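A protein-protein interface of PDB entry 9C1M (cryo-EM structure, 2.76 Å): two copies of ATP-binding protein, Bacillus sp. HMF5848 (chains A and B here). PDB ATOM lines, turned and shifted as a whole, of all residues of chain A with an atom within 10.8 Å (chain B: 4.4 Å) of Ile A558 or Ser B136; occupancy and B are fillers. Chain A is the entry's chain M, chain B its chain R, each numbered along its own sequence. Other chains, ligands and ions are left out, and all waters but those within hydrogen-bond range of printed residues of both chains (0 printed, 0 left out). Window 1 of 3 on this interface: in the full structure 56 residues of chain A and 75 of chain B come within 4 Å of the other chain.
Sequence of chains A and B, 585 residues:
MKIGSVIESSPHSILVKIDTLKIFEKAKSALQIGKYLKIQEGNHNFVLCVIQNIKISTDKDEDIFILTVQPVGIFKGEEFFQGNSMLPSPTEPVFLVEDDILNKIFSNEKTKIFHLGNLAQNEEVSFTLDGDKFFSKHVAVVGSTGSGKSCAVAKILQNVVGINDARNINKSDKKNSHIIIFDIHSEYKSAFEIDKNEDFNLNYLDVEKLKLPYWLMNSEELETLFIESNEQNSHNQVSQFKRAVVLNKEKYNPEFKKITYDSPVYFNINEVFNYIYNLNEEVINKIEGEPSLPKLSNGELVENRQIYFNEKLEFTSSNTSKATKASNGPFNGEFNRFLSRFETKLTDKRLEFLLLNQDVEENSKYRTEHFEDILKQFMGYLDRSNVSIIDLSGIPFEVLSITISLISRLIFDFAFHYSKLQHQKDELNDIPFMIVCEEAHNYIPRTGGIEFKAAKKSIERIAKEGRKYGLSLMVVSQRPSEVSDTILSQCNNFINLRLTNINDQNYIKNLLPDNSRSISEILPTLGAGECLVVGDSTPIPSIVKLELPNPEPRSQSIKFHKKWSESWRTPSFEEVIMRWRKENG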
ATOM      1  N   HIS A 185      -8.754 -15.520  15.595  1.00  0.00           N
ATOM      2  CA  HIS A 185      -9.644 -16.672  15.636  1.00  0.00           C
ATOM      3  C   HIS A 185      -9.161 -17.731  14.646  1.00  0.00           C
ATOM      4  O   HIS A 185      -8.049 -17.662  14.114  1.00  0.00           O
ATOM      5  CB  HIS A 185     -11.084 -16.250  15.357  1.00  0.00           C
ATOM      6  CG  HIS A 185     -11.670 -15.363  16.412  1.00  0.00           C
ATOM      7  ND1 HIS A 185     -11.551 -13.990  16.383  1.00  0.00           N
ATOM      8  CD2 HIS A 185     -12.385 -15.656  17.523  1.00  0.00           C
ATOM      9  CE1 HIS A 185     -12.166 -13.476  17.434  1.00  0.00           C
ATOM     10  NE2 HIS A 185     -12.681 -14.465  18.141  1.00  0.00           N
ATOM     11  N   SER A 186      -9.996 -18.735  14.397  1.00  0.00           N
ATOM     12  CA  SER A 186      -9.704 -19.806  13.451  1.00  0.00           C
ATOM     13  C   SER A 186     -10.587 -19.695  12.211  1.00  0.00           C
ATOM     14  O   SER A 186     -11.030 -20.699  11.649  1.00  0.00           O
ATOM     15  CB  SER A 186      -9.873 -21.171  14.111  1.00  0.00           C
ATOM     16  OG  SER A 186      -9.428 -22.212  13.259  1.00  0.00           O
ATOM     17  N   ARG A 554     -14.525 -19.958   8.019  1.00  0.00           N
ATOM     18  CA  ARG A 554     -15.405 -20.605   8.989  1.00  0.00           C
ATOM     19  C   ARG A 554     -14.576 -20.954  10.212  1.00  0.00           C
ATOM     20  O   ARG A 554     -13.658 -21.776  10.117  1.00  0.00           O
ATOM     21  CB  ARG A 554     -16.036 -21.863   8.387  1.00  0.00           C
ATOM     22  CG  ARG A 554     -16.952 -22.658   9.315  1.00  0.00           C
ATOM     23  CD  ARG A 554     -18.268 -21.941   9.606  1.00  0.00           C
ATOM     24  NE  ARG A 554     -18.200 -20.990  10.710  1.00  0.00           N
ATOM     25  CZ  ARG A 554     -19.176 -20.149  11.026  1.00  0.00           C
ATOM     26  NH1 ARG A 554     -20.309 -20.118  10.343  1.00  0.00           N
ATOM     27  NH2 ARG A 554     -19.015 -19.324  12.056  1.00  0.00           N
ATOM     28  N   SER A 555     -14.886 -20.342  11.351  1.00  0.00           N
ATOM     29  CA  SER A 555     -14.207 -20.664  12.599  1.00  0.00           C
ATOM     30  C   SER A 555     -14.909 -21.836  13.267  1.00  0.00           C
ATOM     31  O   SER A 555     -16.141 -21.865  13.345  1.00  0.00           O
ATOM     32  CB  SER A 555     -14.185 -19.462  13.541  1.00  0.00           C
ATOM     33  OG  SER A 555     -13.229 -19.640  14.573  1.00  0.00           O
ATOM     34  N   GLN A 556     -14.125 -22.795  13.754  1.00  0.00           N
ATOM     35  CA  GLN A 556     -14.703 -23.945  14.436  1.00  0.00           C
ATOM     36  C   GLN A 556     -15.183 -23.544  15.823  1.00  0.00           C
ATOM     37  O   GLN A 556     -14.650 -24.012  16.835  1.00  0.00           O
ATOM     38  CB  GLN A 556     -13.694 -25.091  14.524  1.00  0.00           C
ATOM     39  CG  GLN A 556     -13.353 -25.715  13.182  1.00  0.00           C
ATOM     40  CD  GLN A 556     -12.314 -26.810  13.294  1.00  0.00           C
ATOM     41  OE1 GLN A 556     -11.822 -27.105  14.383  1.00  0.00           O
ATOM     42  NE2 GLN A 556     -11.976 -27.424  12.167  1.00  0.00           N
ATOM     43  N   SER A 557     -16.184 -22.673  15.875  1.00  0.00           N
ATOM     44  CA  SER A 557     -16.779 -22.271  17.135  1.00  0.00           C
ATOM     45  C   SER A 557     -17.748 -23.340  17.625  1.00  0.00           C
ATOM     46  O   SER A 557     -18.246 -24.169  16.859  1.00  0.00           O
ATOM     47  CB  SER A 557     -17.504 -20.933  16.991  1.00  0.00           C
ATOM     48  OG  SER A 557     -16.588 -19.853  16.965  1.00  0.00           O
ATOM     49  N   ILE A 558     -18.012 -23.311  18.925  1.00  0.00           N
ATOM     50  CA  ILE A 558     -18.985 -24.195  19.549  1.00  0.00           C
ATOM     51  C   ILE A 558     -20.258 -23.409  19.822  1.00  0.00           C
ATOM     52  O   ILE A 558     -20.214 -22.293  20.356  1.00  0.00           O
ATOM     53  CB  ILE A 558     -18.423 -24.831  20.834  1.00  0.00           C
ATOM     54  CG1 ILE A 558     -19.357 -25.939  21.325  1.00  0.00           C
ATOM     55  CG2 ILE A 558     -18.114 -23.787  21.904  1.00  0.00           C
ATOM     56  CD1 ILE A 558     -18.749 -26.814  22.369  1.00  0.00           C
ATOM     57  N   LYS A 559     -21.391 -23.973  19.420  1.00  0.00           N
ATOM     58  CA  LYS A 559     -22.696 -23.386  19.686  1.00  0.00           C
ATOM     59  C   LYS A 559     -23.449 -24.291  20.652  1.00  0.00           C
ATOM     60  O   LYS A 559     -23.557 -25.502  20.429  1.00  0.00           O
ATOM     61  CB  LYS A 559     -23.465 -23.149  18.383  1.00  0.00           C
ATOM     62  CG  LYS A 559     -23.853 -24.382  17.602  1.00  0.00           C
ATOM     63  CD  LYS A 559     -24.633 -23.976  16.369  1.00  0.00           C
ATOM     64  CE  LYS A 559     -23.730 -23.327  15.336  1.00  0.00           C
ATOM     65  NZ  LYS A 559     -22.738 -24.295  14.793  1.00  0.00           N
ATOM     66  N   PHE A 560     -23.944 -23.697  21.736  1.00  0.00           N
ATOM     67  CA  PHE A 560     -24.270 -24.450  22.939  1.00  0.00           C
ATOM     68  C   PHE A 560     -25.630 -25.130  22.881  1.00  0.00           C
ATOM     69  O   PHE A 560     -25.858 -26.085  23.631  1.00  0.00           O
ATOM     70  CB  PHE A 560     -24.225 -23.515  24.152  1.00  0.00           C
ATOM     71  CG  PHE A 560     -22.839 -23.263  24.684  1.00  0.00           C
ATOM     72  CD1 PHE A 560     -21.726 -23.443  23.878  1.00  0.00           C
ATOM     73  CD2 PHE A 560     -22.650 -22.823  25.983  1.00  0.00           C
ATOM     74  CE1 PHE A 560     -20.456 -23.200  24.362  1.00  0.00           C
ATOM     75  CE2 PHE A 560     -21.379 -22.580  26.469  1.00  0.00           C
ATOM     76  CZ  PHE A 560     -20.282 -22.768  25.659  1.00  0.00           C
ATOM     77  N   HIS A 561     -26.537 -24.669  22.016  1.00  0.00           N
ATOM     78  CA  HIS A 561     -27.940 -25.046  22.159  1.00  0.00           C
ATOM     79  C   HIS A 561     -28.185 -26.499  21.759  1.00  0.00           C
ATOM     80  O   HIS A 561     -28.859 -27.240  22.484  1.00  0.00           O
ATOM     81  CB  HIS A 561     -28.827 -24.101  21.351  1.00  0.00           C
ATOM     82  CG  HIS A 561     -30.196 -23.922  21.929  1.00  0.00           C
ATOM     83  ND1 HIS A 561     -31.299 -24.600  21.457  1.00  0.00           N
ATOM     84  CD2 HIS A 561     -30.636 -23.151  22.951  1.00  0.00           C
ATOM     85  CE1 HIS A 561     -32.362 -24.248  22.158  1.00  0.00           C
ATOM     86  NE2 HIS A 561     -31.987 -23.370  23.071  1.00  0.00           N
ATOM     87  N   LYS A 562     -27.655 -26.933  20.609  1.00  0.00           N
ATOM     88  CA  LYS A 562     -27.862 -28.328  20.225  1.00  0.00           C
ATOM     89  C   LYS A 562     -27.093 -29.287  21.123  1.00  0.00           C
ATOM     90  O   LYS A 562     -27.566 -30.400  21.379  1.00  0.00           O
ATOM     91  CB  LYS A 562     -27.498 -28.578  18.759  1.00  0.00           C
ATOM     92  CG  LYS A 562     -28.358 -27.838  17.750  1.00  0.00           C
ATOM     93  CD  LYS A 562     -27.959 -28.209  16.327  1.00  0.00           C
ATOM     94  CE  LYS A 562     -26.613 -27.645  15.949  1.00  0.00           C
ATOM     95  NZ  LYS A 562     -26.709 -26.171  15.908  1.00  0.00           N
ATOM     96  N   LYS A 563     -25.916 -28.888  21.608  1.00  0.00           N
ATOM     97  CA  LYS A 563     -25.236 -29.693  22.613  1.00  0.00           C
ATOM     98  C   LYS A 563     -26.054 -29.806  23.891  1.00  0.00           C
ATOM     99  O   LYS A 563     -25.856 -30.749  24.662  1.00  0.00           O
ATOM    100  CB  LYS A 563     -23.856 -29.110  22.922  1.00  0.00           C
ATOM    101  CG  LYS A 563     -22.919 -29.076  21.729  1.00  0.00           C
ATOM    102  CD  LYS A 563     -22.562 -30.486  21.285  1.00  0.00           C
ATOM    103  CE  LYS A 563     -21.585 -30.475  20.123  1.00  0.00           C
ATOM    104  NZ  LYS A 563     -21.293 -31.853  19.637  1.00  0.00           N
ATOM    105  N   TRP A 564     -26.970 -28.868  24.123  1.00  0.00           N
ATOM    106  CA  TRP A 564     -27.852 -28.896  25.280  1.00  0.00           C
ATOM    107  C   TRP A 564     -29.162 -29.621  25.007  1.00  0.00           C
ATOM    108  O   TRP A 564     -29.916 -29.883  25.950  1.00  0.00           O
ATOM    109  CB  TRP A 564     -28.141 -27.465  25.733  1.00  0.00           C
ATOM    110  CG  TRP A 564     -26.983 -26.833  26.423  1.00  0.00           C
ATOM    111  CD1 TRP A 564     -25.761 -27.394  26.649  1.00  0.00           C
ATOM    112  CD2 TRP A 564     -26.910 -25.498  26.927  1.00  0.00           C
ATOM    113  NE1 TRP A 564     -24.941 -26.502  27.292  1.00  0.00           N
ATOM    114  CE2 TRP A 564     -25.623 -25.327  27.470  1.00  0.00           C
ATOM    115  CE3 TRP A 564     -27.813 -24.433  26.983  1.00  0.00           C
ATOM    116  CZ2 TRP A 564     -25.216 -24.138  28.061  1.00  0.00           C
ATOM    117  CZ3 TRP A 564     -27.407 -23.254  27.569  1.00  0.00           C
ATOM    118  CH2 TRP A 564     -26.118 -23.115  28.094  1.00  0.00           C
ATOM    119  N   SER A 565     -29.450 -29.945  23.747  1.00  0.00           N
ATOM    120  CA  SER A 565     -30.650 -30.689  23.391  1.00  0.00           C
ATOM    121  C   SER A 565     -30.453 -32.196  23.463  1.00  0.00           C
ATOM    122  O   SER A 565     -31.427 -32.941  23.310  1.00  0.00           O
ATOM    123  CB  SER A 565     -31.113 -30.306  21.981  1.00  0.00           C
ATOM    124  OG  SER A 565     -30.086 -30.523  21.030  1.00  0.00           O
ATOM    125  N   GLU A 566     -29.227 -32.659  23.688  1.00  0.00           N
ATOM    126  CA  GLU A 566     -28.942 -34.079  23.797  1.00  0.00           C
ATOM    127  C   GLU A 566     -29.078 -34.527  25.250  1.00  0.00           C
ATOM    128  O   GLU A 566     -29.344 -33.731  26.155  1.00  0.00           O
ATOM    129  CB  GLU A 566     -27.551 -34.385  23.246  1.00  0.00           C
ATOM    130  CG  GLU A 566     -27.200 -33.609  21.987  1.00  0.00           C
ATOM    131  CD  GLU A 566     -25.875 -34.037  21.385  1.00  0.00           C
ATOM    132  OE1 GLU A 566     -25.059 -34.643  22.112  1.00  0.00           O
ATOM    133  OE2 GLU A 566     -25.649 -33.768  20.187  1.00  0.00           O
ATOM    134  N   ARG A 569     -24.332 -36.660  28.916  1.00  0.00           N
ATOM    135  CA  ARG A 569     -23.179 -37.333  28.320  1.00  0.00           C
ATOM    136  C   ARG A 569     -22.009 -37.234  29.293  1.00  0.00           C
ATOM    137  O   ARG A 569     -21.378 -36.178  29.412  1.00  0.00           O
ATOM    138  CB  ARG A 569     -22.834 -36.717  26.965  1.00  0.00           C
ATOM    139  CG  ARG A 569     -24.005 -36.669  25.993  1.00  0.00           C
ATOM    140  CD  ARG A 569     -23.549 -36.426  24.562  1.00  0.00           C
ATOM    141  NE  ARG A 569     -22.665 -37.475  24.068  1.00  0.00           N
ATOM    142  CZ  ARG A 569     -22.258 -37.577  22.810  1.00  0.00           C
ATOM    143  NH1 ARG A 569     -22.635 -36.706  21.889  1.00  0.00           N
ATOM    144  NH2 ARG A 569     -21.451 -38.578  22.468  1.00  0.00           N
ATOM    145  N   ASP B 132     -28.698 -20.581  19.504  1.00  0.00           N
ATOM    146  CA  ASP B 132     -27.290 -20.880  19.267  1.00  0.00           C
ATOM    147  C   ASP B 132     -26.427 -19.627  19.332  1.00  0.00           C
ATOM    148  O   ASP B 132     -25.230 -19.713  19.625  1.00  0.00           O
ATOM    149  CB  ASP B 132     -27.119 -21.573  17.915  1.00  0.00           C
ATOM    150  CG  ASP B 132     -27.805 -22.924  17.862  1.00  0.00           C
ATOM    151  OD1 ASP B 132     -27.325 -23.863  18.531  1.00  0.00           O
ATOM    152  OD2 ASP B 132     -28.825 -23.048  17.152  1.00  0.00           O
ATOM    153  N   PHE B 134     -27.255 -17.001  21.360  1.00  0.00           N
ATOM    154  CA  PHE B 134     -27.534 -16.333  22.628  1.00  0.00           C
ATOM    155  C   PHE B 134     -26.676 -16.864  23.771  1.00  0.00           C
ATOM    156  O   PHE B 134     -25.921 -16.106  24.390  1.00  0.00           O
ATOM    157  CB  PHE B 134     -29.022 -16.469  22.980  1.00  0.00           C
ATOM    158  CG  PHE B 134     -29.528 -15.389  23.892  1.00  0.00           C
ATOM    159  CD1 PHE B 134     -29.400 -15.510  25.265  1.00  0.00           C
ATOM    160  CD2 PHE B 134     -30.129 -14.253  23.379  1.00  0.00           C
ATOM    161  CE1 PHE B 134     -29.862 -14.518  26.109  1.00  0.00           C
ATOM    162  CE2 PHE B 134     -30.588 -13.257  24.218  1.00  0.00           C
ATOM    163  CZ  PHE B 134     -30.458 -13.391  25.584  1.00  0.00           C
ATOM    164  N   PHE B 135     -26.774 -18.162  24.066  1.00  0.00           N
ATOM    165  CA  PHE B 135     -26.069 -18.714  25.216  1.00  0.00           C
ATOM    166  C   PHE B 135     -24.626 -19.075  24.898  1.00  0.00           C
ATOM    167  O   PHE B 135     -23.789 -19.113  25.807  1.00  0.00           O
ATOM    168  CB  PHE B 135     -26.808 -19.943  25.749  1.00  0.00           C
ATOM    169  CG  PHE B 135     -28.213 -19.660  26.193  1.00  0.00           C
ATOM    170  CD1 PHE B 135     -28.452 -18.892  27.320  1.00  0.00           C
ATOM    171  CD2 PHE B 135     -29.293 -20.164  25.489  1.00  0.00           C
ATOM    172  CE1 PHE B 135     -29.741 -18.630  27.737  1.00  0.00           C
ATOM    173  CE2 PHE B 135     -30.586 -19.905  25.901  1.00  0.00           C
ATOM    174  CZ  PHE B 135     -30.809 -19.137  27.027  1.00  0.00           C
ATOM    175  N   SER B 136     -24.314 -19.341  23.630  1.00  0.00           N
ATOM    176  CA  SER B 136     -22.955 -19.720  23.264  1.00  0.00           C
ATOM    177  C   SER B 136     -21.972 -18.569  23.419  1.00  0.00           C
ATOM    178  O   SER B 136     -20.761 -18.807  23.482  1.00  0.00           O
ATOM    179  CB  SER B 136     -22.930 -20.238  21.827  1.00  0.00           C
ATOM    180  OG  SER B 136     -23.875 -21.279  21.661  1.00  0.00           O
ATOM    181  N   LYS B 137     -22.461 -17.336  23.483  1.00  0.00           N
ATOM    182  CA  LYS B 137     -21.627 -16.153  23.618  1.00  0.00           C
ATOM    183  C   LYS B 137     -21.888 -15.482  24.960  1.00  0.00           C
ATOM    184  O   LYS B 137     -22.955 -15.637  25.561  1.00  0.00           O
ATOM    185  CB  LYS B 137     -21.891 -15.170  22.471  1.00  0.00           C
ATOM    186  CG  LYS B 137     -21.920 -15.831  21.101  1.00  0.00           C
ATOM    187  CD  LYS B 137     -21.726 -14.820  19.983  1.00  0.00           C
ATOM    188  CE  LYS B 137     -23.055 -14.248  19.521  1.00  0.00           C
ATOM    189  NZ  LYS B 137     -22.903 -13.396  18.310  1.00  0.00           N
ATOM    190  N   ASN B 429     -15.672 -29.686  21.860  1.00  0.00           N
ATOM    191  CA  ASN B 429     -16.274 -29.904  23.168  1.00  0.00           C
ATOM    192  C   ASN B 429     -17.710 -30.400  23.030  1.00  0.00           C
ATOM    193  O   ASN B 429     -18.487 -29.900  22.213  1.00  0.00           O
ATOM    194  CB  ASN B 429     -16.226 -28.605  23.979  1.00  0.00           C
ATOM    195  CG  ASN B 429     -16.648 -28.787  25.428  1.00  0.00           C
ATOM    196  OD1 ASN B 429     -17.013 -29.880  25.854  1.00  0.00           O
ATOM    197  ND2 ASN B 429     -16.590 -27.705  26.194  1.00  0.00           N
ATOM    198  N   PRO B 432     -20.426 -28.203  27.058  1.00  0.00           N
ATOM    199  CA  PRO B 432     -20.193 -26.793  27.385  1.00  0.00           C
ATOM    200  C   PRO B 432     -20.656 -26.477  28.799  1.00  0.00           C
ATOM    201  O   PRO B 432     -21.258 -27.299  29.491  1.00  0.00           O
ATOM    202  CB  PRO B 432     -21.036 -26.051  26.348  1.00  0.00           C
ATOM    203  CG  PRO B 432     -21.151 -26.995  25.210  1.00  0.00           C
ATOM    204  CD  PRO B 432     -21.219 -28.358  25.825  1.00  0.00           C
ATOM    205  N   ARG B 467     -14.711 -19.183  24.674  1.00  0.00           N
ATOM    206  CA  ARG B 467     -15.617 -19.468  23.569  1.00  0.00           C
ATOM    207  C   ARG B 467     -15.056 -20.556  22.666  1.00  0.00           C
ATOM    208  O   ARG B 467     -15.821 -21.304  22.047  1.00  0.00           O
ATOM    209  CB  ARG B 467     -15.893 -18.191  22.775  1.00  0.00           C
ATOM    210  CG  ARG B 467     -16.710 -17.160  23.541  1.00  0.00           C
ATOM    211  CD  ARG B 467     -17.132 -16.001  22.653  1.00  0.00           C
ATOM    212  NE  ARG B 467     -15.986 -15.244  22.160  1.00  0.00           N
ATOM    213  CZ  ARG B 467     -15.432 -14.226  22.804  1.00  0.00           C
ATOM    214  NH1 ARG B 467     -15.892 -13.814  23.973  1.00  0.00           N
ATOM    215  NH2 ARG B 467     -14.389 -13.605  22.259  1.00  0.00           N
ATOM    216  N   GLY B 470     -15.382 -23.828  25.086  1.00  0.00           N
ATOM    217  CA  GLY B 470     -16.704 -24.192  25.559  1.00  0.00           C
ATOM    218  C   GLY B 470     -17.084 -23.632  26.914  1.00  0.00           C
ATOM    219  O   GLY B 470     -17.387 -24.393  27.838  1.00  0.00           O
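The backbone NH (N) of Phe A560 lies within hydrogen-bond range of the side-chain hydroxyl (OG) of Ser B136 (2.4 Å). The side-chain amino group of Lys A562 is in salt-bridge range of the side-chain carboxylate of Asp B132.
The side-chain hydroxyl of Ser A565 lies within hydrogen-bond range of the backbone carbonyl oxygen of Lys A562 (2.5 Å). The backbone carbonyl oxygen (O) of Asp B132 sits at hydrogen-bond distance from the side-chain hydroxyl (OG) of Ser B136, at 2.9 Å.
Among the printed residues, pairs that only touch across the chains: Ile A558 with Ser B136 (3.7 Å), Ile A558 with Asn B429 (3.1 Å), Ile A558 with Pro B432 (3.7 Å), Ile A558 with Arg B467 (3.4 Å), Ile A558 with Gly B470 (3.9 Å), Lys A559 with Asp B132 (3.5 Å), Lys A559 with Ser B136 (3.1 Å), Phe A560 with Phe B135 (3.9 Å), Phe A560 with Pro B432 (3.4 Å), Phe A560 with Gly B470 (3.5 Å), His A561 with Asp B132 (3.2 Å), Lys A563 with Asn B429 (3.8 Å), Lys A563 with Pro B432 (3.99 Å) and Trp A564 with Phe B135 (3.8 Å).
Of chain B, only Ser B136 (3.7 Å), Asn B429 (3.1 Å), Pro B432 (3.7 Å), Arg B467 (3.4 Å) and Gly B470 (3.9 Å) come within 4 Å of Ile A558. Of the printed residues of chain B, His A561 touches Asp B132. Ser A565 touches none of the printed residues of chain B. Arg A569 touches none of the printed residues of chain B. Printed residues of chain A within 4 Å of Phe B135: Phe A560 and Trp A564. Printed residues of chain A within 4 Å of Ser B136: Ile A558 (3.7 Å), Lys A559 (3.1 Å) and Phe A560 (2.4 Å). Asn B429 touches just these residues of chain A: Ile A558 and Lys A563. Printed residues of chain A within 4 Å of Pro B432: Ile A558 (3.7 Å), Phe A560 (3.4 Å) and Lys A563 (3.99 Å). Of chain A, only Ile A558 and Phe A560 come within 4 Å of Gly B470. The nearest printed residue of chain A that does not touch Asp B132 is Phe A560 (4.7 Å).
Hydrophobic or aromatic side chains of chain A within 4 Å of the printed part of chain B: Ile A558, Phe A560, His A561 and Trp A564. Of the 9 printed residues of chain B, 7 touch a printed residue of chain A. Hydrophobic or aromatic side chains of chain B within 4 Å of the printed part of chain A: Phe B135 and Pro B432. Along chain B the printed residues that touch a printed residue of chain A span positions 132 to 470. Among the printed residues, Asp or Glu carboxylates within 4 Å of a Lys or Arg side-chain nitrogen of the other chain: Lys A562 with Asp B132 (3.5 Å).
No position is printed for both chains. Of the 16 pairs that touch across the chains among the printed residues, none has its exchanged pair printed and touching as well.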
